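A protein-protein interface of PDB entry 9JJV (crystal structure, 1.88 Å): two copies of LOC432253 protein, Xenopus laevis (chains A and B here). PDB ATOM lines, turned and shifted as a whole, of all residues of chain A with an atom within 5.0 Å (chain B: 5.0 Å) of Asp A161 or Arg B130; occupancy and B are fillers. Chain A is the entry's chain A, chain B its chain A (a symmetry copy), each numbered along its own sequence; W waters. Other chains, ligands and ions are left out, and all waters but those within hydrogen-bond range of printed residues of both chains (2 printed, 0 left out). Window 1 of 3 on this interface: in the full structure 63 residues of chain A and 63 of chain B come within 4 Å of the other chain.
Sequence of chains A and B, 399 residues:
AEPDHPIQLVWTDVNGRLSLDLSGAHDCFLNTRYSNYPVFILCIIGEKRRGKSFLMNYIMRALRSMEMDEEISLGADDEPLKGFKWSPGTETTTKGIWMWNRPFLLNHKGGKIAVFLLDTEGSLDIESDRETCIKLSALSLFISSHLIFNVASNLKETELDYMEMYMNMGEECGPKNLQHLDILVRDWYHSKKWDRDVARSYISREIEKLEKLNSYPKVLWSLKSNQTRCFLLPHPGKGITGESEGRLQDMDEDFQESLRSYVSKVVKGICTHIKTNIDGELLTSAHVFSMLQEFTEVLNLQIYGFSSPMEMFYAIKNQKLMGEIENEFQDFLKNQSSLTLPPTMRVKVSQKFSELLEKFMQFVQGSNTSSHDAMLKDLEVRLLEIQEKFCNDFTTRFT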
ATOM      1  N   LYS A 156       4.191 -26.698  -7.400  1.00  0.00           N
ATOM      2  CA  LYS A 156       5.533 -27.167  -7.688  1.00  0.00           C
ATOM      3  C   LYS A 156       6.328 -26.001  -8.241  1.00  0.00           C
ATOM      4  O   LYS A 156       5.811 -24.901  -8.442  1.00  0.00           O
ATOM      5  CB  LYS A 156       5.555 -28.298  -8.726  1.00  0.00           C
ATOM      6  CG  LYS A 156       4.510 -29.329  -8.524  1.00  0.00           C
ATOM      7  CD  LYS A 156       4.559 -30.405  -9.592  1.00  0.00           C
ATOM      8  CE  LYS A 156       3.759 -30.002 -10.793  1.00  0.00           C
ATOM      9  NZ  LYS A 156       2.388 -29.569 -10.409  1.00  0.00           N
ATOM     10  N   GLU A 157       7.597 -26.263  -8.500  1.00  0.00           N
ATOM     11  CA  GLU A 157       8.447 -25.271  -9.147  1.00  0.00           C
ATOM     12  C   GLU A 157       7.771 -24.618 -10.348  1.00  0.00           C
ATOM     13  O   GLU A 157       7.771 -23.383 -10.480  1.00  0.00           O
ATOM     14  CB  GLU A 157       9.752 -25.952  -9.545  1.00  0.00           C
ATOM     15  CG  GLU A 157      10.705 -25.141 -10.396  1.00  0.00           C
ATOM     16  CD  GLU A 157      11.757 -26.055 -11.042  1.00  0.00           C
ATOM     17  OE1 GLU A 157      11.659 -26.476 -12.233  1.00  0.00           O
ATOM     18  OE2 GLU A 157      12.645 -26.437 -10.258  1.00  0.00           O
ATOM     19  N   THR A 158       7.153 -25.420 -11.224  1.00  0.00           N
ATOM     20  CA  THR A 158       6.589 -24.859 -12.458  1.00  0.00           C
ATOM     21  C   THR A 158       5.535 -23.806 -12.191  1.00  0.00           C
ATOM     22  O   THR A 158       5.493 -22.779 -12.875  1.00  0.00           O
ATOM     23  CB  THR A 158       5.986 -25.961 -13.323  1.00  0.00           C
ATOM     24  OG1 THR A 158       6.866 -27.088 -13.297  1.00  0.00           O
ATOM     25  CG2 THR A 158       5.799 -25.464 -14.747  1.00  0.00           C
ATOM     26  N   GLU A 159       4.592 -24.098 -11.291  1.00  0.00           N
ATOM     27  CA  GLU A 159       3.524 -23.146 -11.018  1.00  0.00           C
ATOM     28  C   GLU A 159       4.057 -21.882 -10.390  1.00  0.00           C
ATOM     29  O   GLU A 159       3.584 -20.787 -10.707  1.00  0.00           O
ATOM     30  CB  GLU A 159       2.477 -23.759 -10.089  1.00  0.00           C
ATOM     31  CG  GLU A 159       1.617 -24.761 -10.775  1.00  0.00           C
ATOM     32  CD  GLU A 159       2.277 -26.106 -10.766  1.00  0.00           C
ATOM     33  OE1 GLU A 159       3.188 -26.320  -9.932  1.00  0.00           O
ATOM     34  OE2 GLU A 159       1.869 -26.960 -11.576  1.00  0.00           O
ATOM     35  N   LEU A 160       4.999 -22.014  -9.453  1.00  0.00           N
ATOM     36  CA  LEU A 160       5.579 -20.828  -8.828  1.00  0.00           C
ATOM     37  C   LEU A 160       6.397 -20.028  -9.836  1.00  0.00           C
ATOM     38  O   LEU A 160       6.312 -18.790  -9.866  1.00  0.00           O
ATOM     39  CB  LEU A 160       6.432 -21.257  -7.627  1.00  0.00           C
ATOM     40  CG  LEU A 160       5.538 -22.030  -6.647  1.00  0.00           C
ATOM     41  CD1 LEU A 160       6.316 -22.574  -5.474  1.00  0.00           C
ATOM     42  CD2 LEU A 160       4.429 -21.116  -6.157  1.00  0.00           C
ATOM     43  N   ASP A 161       7.192 -20.722 -10.676  1.00  0.00           N
ATOM     44  CA  ASP A 161       7.921 -20.065 -11.764  1.00  0.00           C
ATOM     45  C   ASP A 161       6.982 -19.222 -12.622  1.00  0.00           C
ATOM     46  O   ASP A 161       7.281 -18.062 -12.957  1.00  0.00           O
ATOM     47  CB  ASP A 161       8.592 -21.110 -12.672  1.00  0.00           C
ATOM     48  CG  ASP A 161       9.880 -21.686 -12.114  1.00  0.00           C
ATOM     49  OD1 ASP A 161      10.349 -21.246 -11.039  1.00  0.00           O
ATOM     50  OD2 ASP A 161      10.433 -22.604 -12.803  1.00  0.00           O
ATOM     51  N   TYR A 162       5.852 -19.817 -13.039  1.00  0.00           N
ATOM     52  CA  TYR A 162       4.973 -19.140 -13.989  1.00  0.00           C
ATOM     53  C   TYR A 162       4.195 -18.018 -13.328  1.00  0.00           C
ATOM     54  O   TYR A 162       4.077 -16.926 -13.895  1.00  0.00           O
ATOM     55  CB  TYR A 162       4.024 -20.138 -14.670  1.00  0.00           C
ATOM     56  CG  TYR A 162       4.609 -20.657 -15.957  1.00  0.00           C
ATOM     57  CD1 TYR A 162       4.400 -19.972 -17.146  1.00  0.00           C
ATOM     58  CD2 TYR A 162       5.439 -21.775 -15.974  1.00  0.00           C
ATOM     59  CE1 TYR A 162       4.973 -20.410 -18.340  1.00  0.00           C
ATOM     60  CE2 TYR A 162       6.007 -22.228 -17.164  1.00  0.00           C
ATOM     61  CZ  TYR A 162       5.754 -21.533 -18.343  1.00  0.00           C
ATOM     62  OH  TYR A 162       6.320 -21.948 -19.530  1.00  0.00           O
ATOM     63  N   MET A 163       3.675 -18.239 -12.119  1.00  0.00           N
ATOM     64  CA  MET A 163       2.940 -17.137 -11.522  1.00  0.00           C
ATOM     65  C   MET A 163       3.859 -15.971 -11.168  1.00  0.00           C
ATOM     66  O   MET A 163       3.445 -14.809 -11.280  1.00  0.00           O
ATOM     67  CB  MET A 163       2.112 -17.618 -10.323  1.00  0.00           C
ATOM     68  CG  MET A 163       1.412 -16.446  -9.614  1.00  0.00           C
ATOM     69  SD  MET A 163       0.051 -15.739 -10.595  1.00  0.00           S
ATOM     70  CE  MET A 163      -1.200 -17.025 -10.595  1.00  0.00           C
ATOM     71  N   GLU A 164       5.117 -16.246 -10.800  1.00  0.00           N
ATOM     72  CA  GLU A 164       6.058 -15.149 -10.604  1.00  0.00           C
ATOM     73  C   GLU A 164       6.256 -14.390 -11.907  1.00  0.00           C
ATOM     74  O   GLU A 164       6.331 -13.154 -11.914  1.00  0.00           O
ATOM     75  CB  GLU A 164       7.398 -15.679 -10.091  1.00  0.00           C
ATOM     76  CG  GLU A 164       8.337 -14.695  -9.327  1.00  0.00           C
ATOM     77  CD  GLU A 164       7.760 -14.061  -8.044  1.00  0.00           C
ATOM     78  OE1 GLU A 164       8.217 -12.951  -7.663  1.00  0.00           O
ATOM     79  OE2 GLU A 164       6.886 -14.676  -7.374  1.00  0.00           O
ATOM     80  N   MET A 165       6.309 -15.108 -13.025  1.00  0.00           N
ATOM     81  CA  MET A 165       6.439 -14.426 -14.308  1.00  0.00           C
ATOM     82  C   MET A 165       5.211 -13.568 -14.590  1.00  0.00           C
ATOM     83  O   MET A 165       5.330 -12.385 -14.964  1.00  0.00           O
ATOM     84  CB  MET A 165       6.629 -15.415 -15.448  1.00  0.00           C
ATOM     85  CG  MET A 165       8.030 -15.988 -15.521  1.00  0.00           C
ATOM     86  SD  MET A 165       8.389 -16.821 -17.066  1.00  0.00           S
ATOM     87  CE  MET A 165       7.437 -18.327 -16.854  1.00  0.00           C
ATOM     88  N   TYR A 216      10.647 -16.256  -5.334  1.00  0.00           N
ATOM     89  CA  TYR A 216       9.224 -15.975  -5.554  1.00  0.00           C
ATOM     90  C   TYR A 216       8.705 -14.916  -4.592  1.00  0.00           C
ATOM     91  O   TYR A 216       7.728 -15.146  -3.869  1.00  0.00           O
ATOM     92  CB  TYR A 216       8.410 -17.258  -5.416  1.00  0.00           C
ATOM     93  CG  TYR A 216       8.978 -18.438  -6.184  1.00  0.00           C
ATOM     94  CD1 TYR A 216       8.968 -18.438  -7.560  1.00  0.00           C
ATOM     95  CD2 TYR A 216       9.498 -19.550  -5.521  1.00  0.00           C
ATOM     96  CE1 TYR A 216       9.481 -19.500  -8.284  1.00  0.00           C
ATOM     97  CE2 TYR A 216      10.005 -20.651  -6.235  1.00  0.00           C
ATOM     98  CZ  TYR A 216       9.973 -20.611  -7.616  1.00  0.00           C
ATOM     99  OH  TYR A 216      10.450 -21.661  -8.361  1.00  0.00           O
ATOM    100  N   SER B 128      14.640 -27.794  -2.953  1.00  0.00           N
ATOM    101  CA  SER B 128      15.864 -28.372  -3.470  1.00  0.00           C
ATOM    102  C   SER B 128      16.355 -27.472  -4.591  1.00  0.00           C
ATOM    103  O   SER B 128      15.552 -26.975  -5.391  1.00  0.00           O
ATOM    104  CB  SER B 128      15.591 -29.796  -3.970  1.00  0.00           C
ATOM    105  OG  SER B 128      16.706 -30.640  -3.813  1.00  0.00           O
ATOM    106  N   ASP B 129      17.662 -27.223  -4.638  1.00  0.00           N
ATOM    107  CA  ASP B 129      18.216 -26.420  -5.726  1.00  0.00           C
ATOM    108  C   ASP B 129      18.037 -27.163  -7.038  1.00  0.00           C
ATOM    109  O   ASP B 129      18.474 -28.313  -7.160  1.00  0.00           O
ATOM    110  CB  ASP B 129      19.693 -26.120  -5.476  1.00  0.00           C
ATOM    111  CG  ASP B 129      20.197 -24.945  -6.298  1.00  0.00           C
ATOM    112  OD1 ASP B 129      19.941 -24.904  -7.531  1.00  0.00           O
ATOM    113  OD2 ASP B 129      20.807 -24.027  -5.701  1.00  0.00           O
ATOM    114  N   ARG B 130      17.400 -26.517  -8.025  1.00  0.00           N
ATOM    115  CA  ARG B 130      17.014 -27.265  -9.221  1.00  0.00           C
ATOM    116  C   ARG B 130      18.225 -27.781  -9.980  1.00  0.00           C
ATOM    117  O   ARG B 130      18.157 -28.848 -10.602  1.00  0.00           O
ATOM    118  CB  ARG B 130      16.098 -26.425 -10.123  1.00  0.00           C
ATOM    119  CG  ARG B 130      16.771 -25.333 -10.951  1.00  0.00           C
ATOM    120  CD  ARG B 130      15.717 -24.555 -11.774  1.00  0.00           C
ATOM    121  NE  ARG B 130      14.911 -23.714 -10.896  1.00  0.00           N
ATOM    122  CZ  ARG B 130      13.717 -23.221 -11.198  1.00  0.00           C
ATOM    123  NH1 ARG B 130      13.146 -23.460 -12.366  1.00  0.00           N
ATOM    124  NH2 ARG B 130      13.081 -22.471 -10.300  1.00  0.00           N
ATOM    125  N   GLU B 131      19.352 -27.077  -9.919  1.00  0.00           N
ATOM    126  CA  GLU B 131      20.528 -27.589 -10.612  1.00  0.00           C
ATOM    127  C   GLU B 131      21.019 -28.880  -9.961  1.00  0.00           C
ATOM    128  O   GLU B 131      21.460 -29.815 -10.643  1.00  0.00           O
ATOM    129  CB  GLU B 131      21.644 -26.539 -10.620  1.00  0.00           C
ATOM    130  CG  GLU B 131      22.911 -27.040 -11.299  1.00  0.00           C
ATOM    131  CD  GLU B 131      23.843 -25.922 -11.733  1.00  0.00           C
ATOM    132  OE1 GLU B 131      23.350 -24.787 -11.957  1.00  0.00           O
ATOM    133  OE2 GLU B 131      25.065 -26.199 -11.870  1.00  0.00           O
ATOM    134  N   THR B 132      20.940 -28.939  -8.640  1.00  0.00           N
ATOM    135  CA  THR B 132      21.341 -30.131  -7.909  1.00  0.00           C
ATOM    136  C   THR B 132      20.529 -31.356  -8.341  1.00  0.00           C
ATOM    137  O   THR B 132      21.090 -32.420  -8.641  1.00  0.00           O
ATOM    138  CB  THR B 132      21.182 -29.836  -6.418  1.00  0.00           C
ATOM    139  OG1 THR B 132      22.267 -28.995  -6.009  1.00  0.00           O
ATOM    140  CG2 THR B 132      21.209 -31.077  -5.643  1.00  0.00           C
ATOM    141  N   CYS B 133      19.204 -31.222  -8.408  1.00  0.00           N
ATOM    142  CA  CYS B 133      18.391 -32.340  -8.886  1.00  0.00           C
ATOM    143  C   CYS B 133      18.632 -32.641 -10.358  1.00  0.00           C
ATOM    144  O   CYS B 133      18.515 -33.800 -10.786  1.00  0.00           O
ATOM    145  CB  CYS B 133      16.912 -32.067  -8.639  1.00  0.00           C
ATOM    146  SG  CYS B 133      15.915 -33.564  -8.916  1.00  0.00           S
ATOM    147  N   ILE B 134      18.977 -31.628 -11.158  1.00  0.00           N
ATOM    148  CA  ILE B 134      19.314 -31.888 -12.549  1.00  0.00           C
ATOM    149  C   ILE B 134      20.557 -32.770 -12.636  1.00  0.00           C
ATOM    150  O   ILE B 134      20.633 -33.694 -13.463  1.00  0.00           O
ATOM    151  CB  ILE B 134      19.497 -30.555 -13.297  1.00  0.00           C
ATOM    152  CG1 ILE B 134      18.119 -29.911 -13.520  1.00  0.00           C
ATOM    153  CG2 ILE B 134      20.237 -30.757 -14.620  1.00  0.00           C
ATOM    154  CD1 ILE B 134      18.201 -28.407 -13.827  1.00  0.00           C
ATOM    155  N   TYR B 162      13.316 -30.441 -19.259  1.00  0.00           N
ATOM    156  CA  TYR B 162      14.222 -31.094 -18.317  1.00  0.00           C
ATOM    157  C   TYR B 162      15.010 -32.208 -18.981  1.00  0.00           C
ATOM    158  O   TYR B 162      16.220 -32.329 -18.761  1.00  0.00           O
ATOM    159  CB  TYR B 162      13.458 -31.618 -17.091  1.00  0.00           C
ATOM    160  CG  TYR B 162      13.438 -30.598 -15.983  1.00  0.00           C
ATOM    161  CD1 TYR B 162      14.469 -30.552 -15.057  1.00  0.00           C
ATOM    162  CD2 TYR B 162      12.439 -29.630 -15.914  1.00  0.00           C
ATOM    163  CE1 TYR B 162      14.492 -29.585 -14.053  1.00  0.00           C
ATOM    164  CE2 TYR B 162      12.447 -28.665 -14.907  1.00  0.00           C
ATOM    165  CZ  TYR B 162      13.482 -28.664 -13.976  1.00  0.00           C
ATOM    166  OH  TYR B 162      13.525 -27.709 -12.982  1.00  0.00           O
ATOM    167  N   PHE B 306      21.365 -22.693 -13.467  1.00  0.00           N
ATOM    168  CA  PHE B 306      19.935 -22.878 -13.694  1.00  0.00           C
ATOM    169  C   PHE B 306      19.155 -22.264 -12.545  1.00  0.00           C
ATOM    170  O   PHE B 306      19.497 -22.442 -11.377  1.00  0.00           O
ATOM    171  CB  PHE B 306      19.563 -24.361 -13.795  1.00  0.00           C
ATOM    172  CG  PHE B 306      20.249 -25.098 -14.913  1.00  0.00           C
ATOM    173  CD1 PHE B 306      20.159 -24.654 -16.212  1.00  0.00           C
ATOM    174  CD2 PHE B 306      20.966 -26.252 -14.648  1.00  0.00           C
ATOM    175  CE1 PHE B 306      20.789 -25.334 -17.233  1.00  0.00           C
ATOM    176  CE2 PHE B 306      21.589 -26.944 -15.660  1.00  0.00           C
ATOM    177  CZ  PHE B 306      21.500 -26.484 -16.953  1.00  0.00           C
ATOM    178  N   SER B 307      18.098 -21.561 -12.906  1.00  0.00           N
ATOM    179  CA  SER B 307      17.251 -20.908 -11.889  1.00  0.00           C
ATOM    180  C   SER B 307      15.862 -20.683 -12.472  1.00  0.00           C
ATOM    181  O   SER B 307      15.579 -21.227 -13.525  1.00  0.00           O
ATOM    182  CB  SER B 307      17.873 -19.618 -11.461  1.00  0.00           C
ATOM    183  OG  SER B 307      17.945 -18.713 -12.549  1.00  0.00           O
ATOM    184  N   SER B 308      15.051 -19.880 -11.787  1.00  0.00           N
ATOM    185  CA  SER B 308      13.692 -19.539 -12.273  1.00  0.00           C
ATOM    186  C   SER B 308      13.787 -18.806 -13.607  1.00  0.00           C
ATOM    187  O   SER B 308      14.756 -18.088 -13.827  1.00  0.00           O
ATOM    188  CB  SER B 308      12.943 -18.704 -11.263  1.00  0.00           C
ATOM    189  OG  SER B 308      13.422 -17.376 -11.229  1.00  0.00           O
ATOM    190  N   PRO B 309      12.787 -18.963 -14.487  1.00  0.00           N
ATOM    191  CA  PRO B 309      12.786 -18.270 -15.770  1.00  0.00           C
ATOM    192  C   PRO B 309      12.890 -16.739 -15.632  1.00  0.00           C
ATOM    193  O   PRO B 309      13.544 -16.131 -16.429  1.00  0.00           O
ATOM    194  CB  PRO B 309      11.444 -18.695 -16.391  1.00  0.00           C
ATOM    195  CG  PRO B 309      10.627 -19.235 -15.249  1.00  0.00           C
ATOM    196  CD  PRO B 309      11.641 -19.841 -14.308  1.00  0.00           C
HETATM  197  O   HOH W   1      13.587 -29.046  -9.971  1.00  0.00           O
HETATM  198  O   HOH W   2      12.347 -23.241  -7.259  1.00  0.00           O
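The guanidinium group of Arg B130 lies within salt-bridge range of the side-chain carboxylate of Glu A157 (3.4 Å).
OE2 of Glu A157 lies close to OH of Tyr B162, at 3.1 Å.
The side-chain carboxylate of Asp A161 lies within salt-bridge range of the guanidinium group of Arg B130, 2.9 Å away.
The side-chain hydroxyl of Tyr A216 is in hydrogen-bond range of the guanidinium group of Arg B130, 3.4 Å away.
OD1 of Asp A161 sits at hydrogen-bond distance from OH of Tyr A216, 2.7 Å away.
The backbone carbonyl oxygen (O) of Ser B307 lies within hydrogen-bond range of the guanidinium group (NH1) of Arg B130 (3.5 Å).
Among the printed residues, pairs that only touch across the chains: Asp A161 with Pro B309 (3.4 Å), Asp A161 with Ser B308 (3.6 Å) and Met A165 with Pro B309 (3.6 Å).
Asp A161 touches just these residues of chain B: Arg B130 (2.9 Å), Ser B308 (3.6 Å) and Pro B309 (3.4 Å).
Arg B130 touches just these residues of chain A: Glu A157, Asp A161 and Tyr A216.
Of the printed residues of chain A, Tyr B162 touches Glu A157 (2.4 Å).
Of the printed residues of chain B, Met A165 touches Pro B309 (3.6 Å).
Of the printed residues of chain A, Pro B309 touches Asp A161 and Met A165.
Of the printed residues of chain B, Glu A157 touches Arg B130 (3.2 Å) and Tyr B162 (2.4 Å).
Met A163 touches none of the printed residues of chain B.
The nearest printed residue of chain B that does not touch Asp A161 is Ser B307 (5.4 Å).
The nearest printed residue of chain A that does not touch Tyr B162 is Asp A161 (6.0 Å).
Of the 11 printed residues of chain A, 4 touch a printed residue of chain B.
Hydrophobic or aromatic side chains of chain A that line the printed part of chain B: Met A165 and Tyr A216.
Along chain A the printed residues that touch a printed residue of chain B span positions 157 to 216.
Of the 12 printed residues of chain B, 4 touch a printed residue of chain A.
Hydrophobic or aromatic side chains of chain B within 4 Å of the printed part of chain A: Tyr B162 and Pro B309.
Among the printed residues, 7 pairs touch across the chains.
1 position is printed for both chains.
Of the 7 pairs that touch across the chains among the printed residues, none has its exchanged pair printed and touching as well.
Water W2 bridges the side-chain hydroxyl (OH) of Tyr A216 (2.7 Å) and the guanidinium group (NH2) of Arg B130 (3.2 Å).
Water W1 lies within hydrogen-bond range of the side-chain carboxylate of Glu A157 (2.8 Å) and the side-chain hydroxyl of Tyr B162 (3.3 Å).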
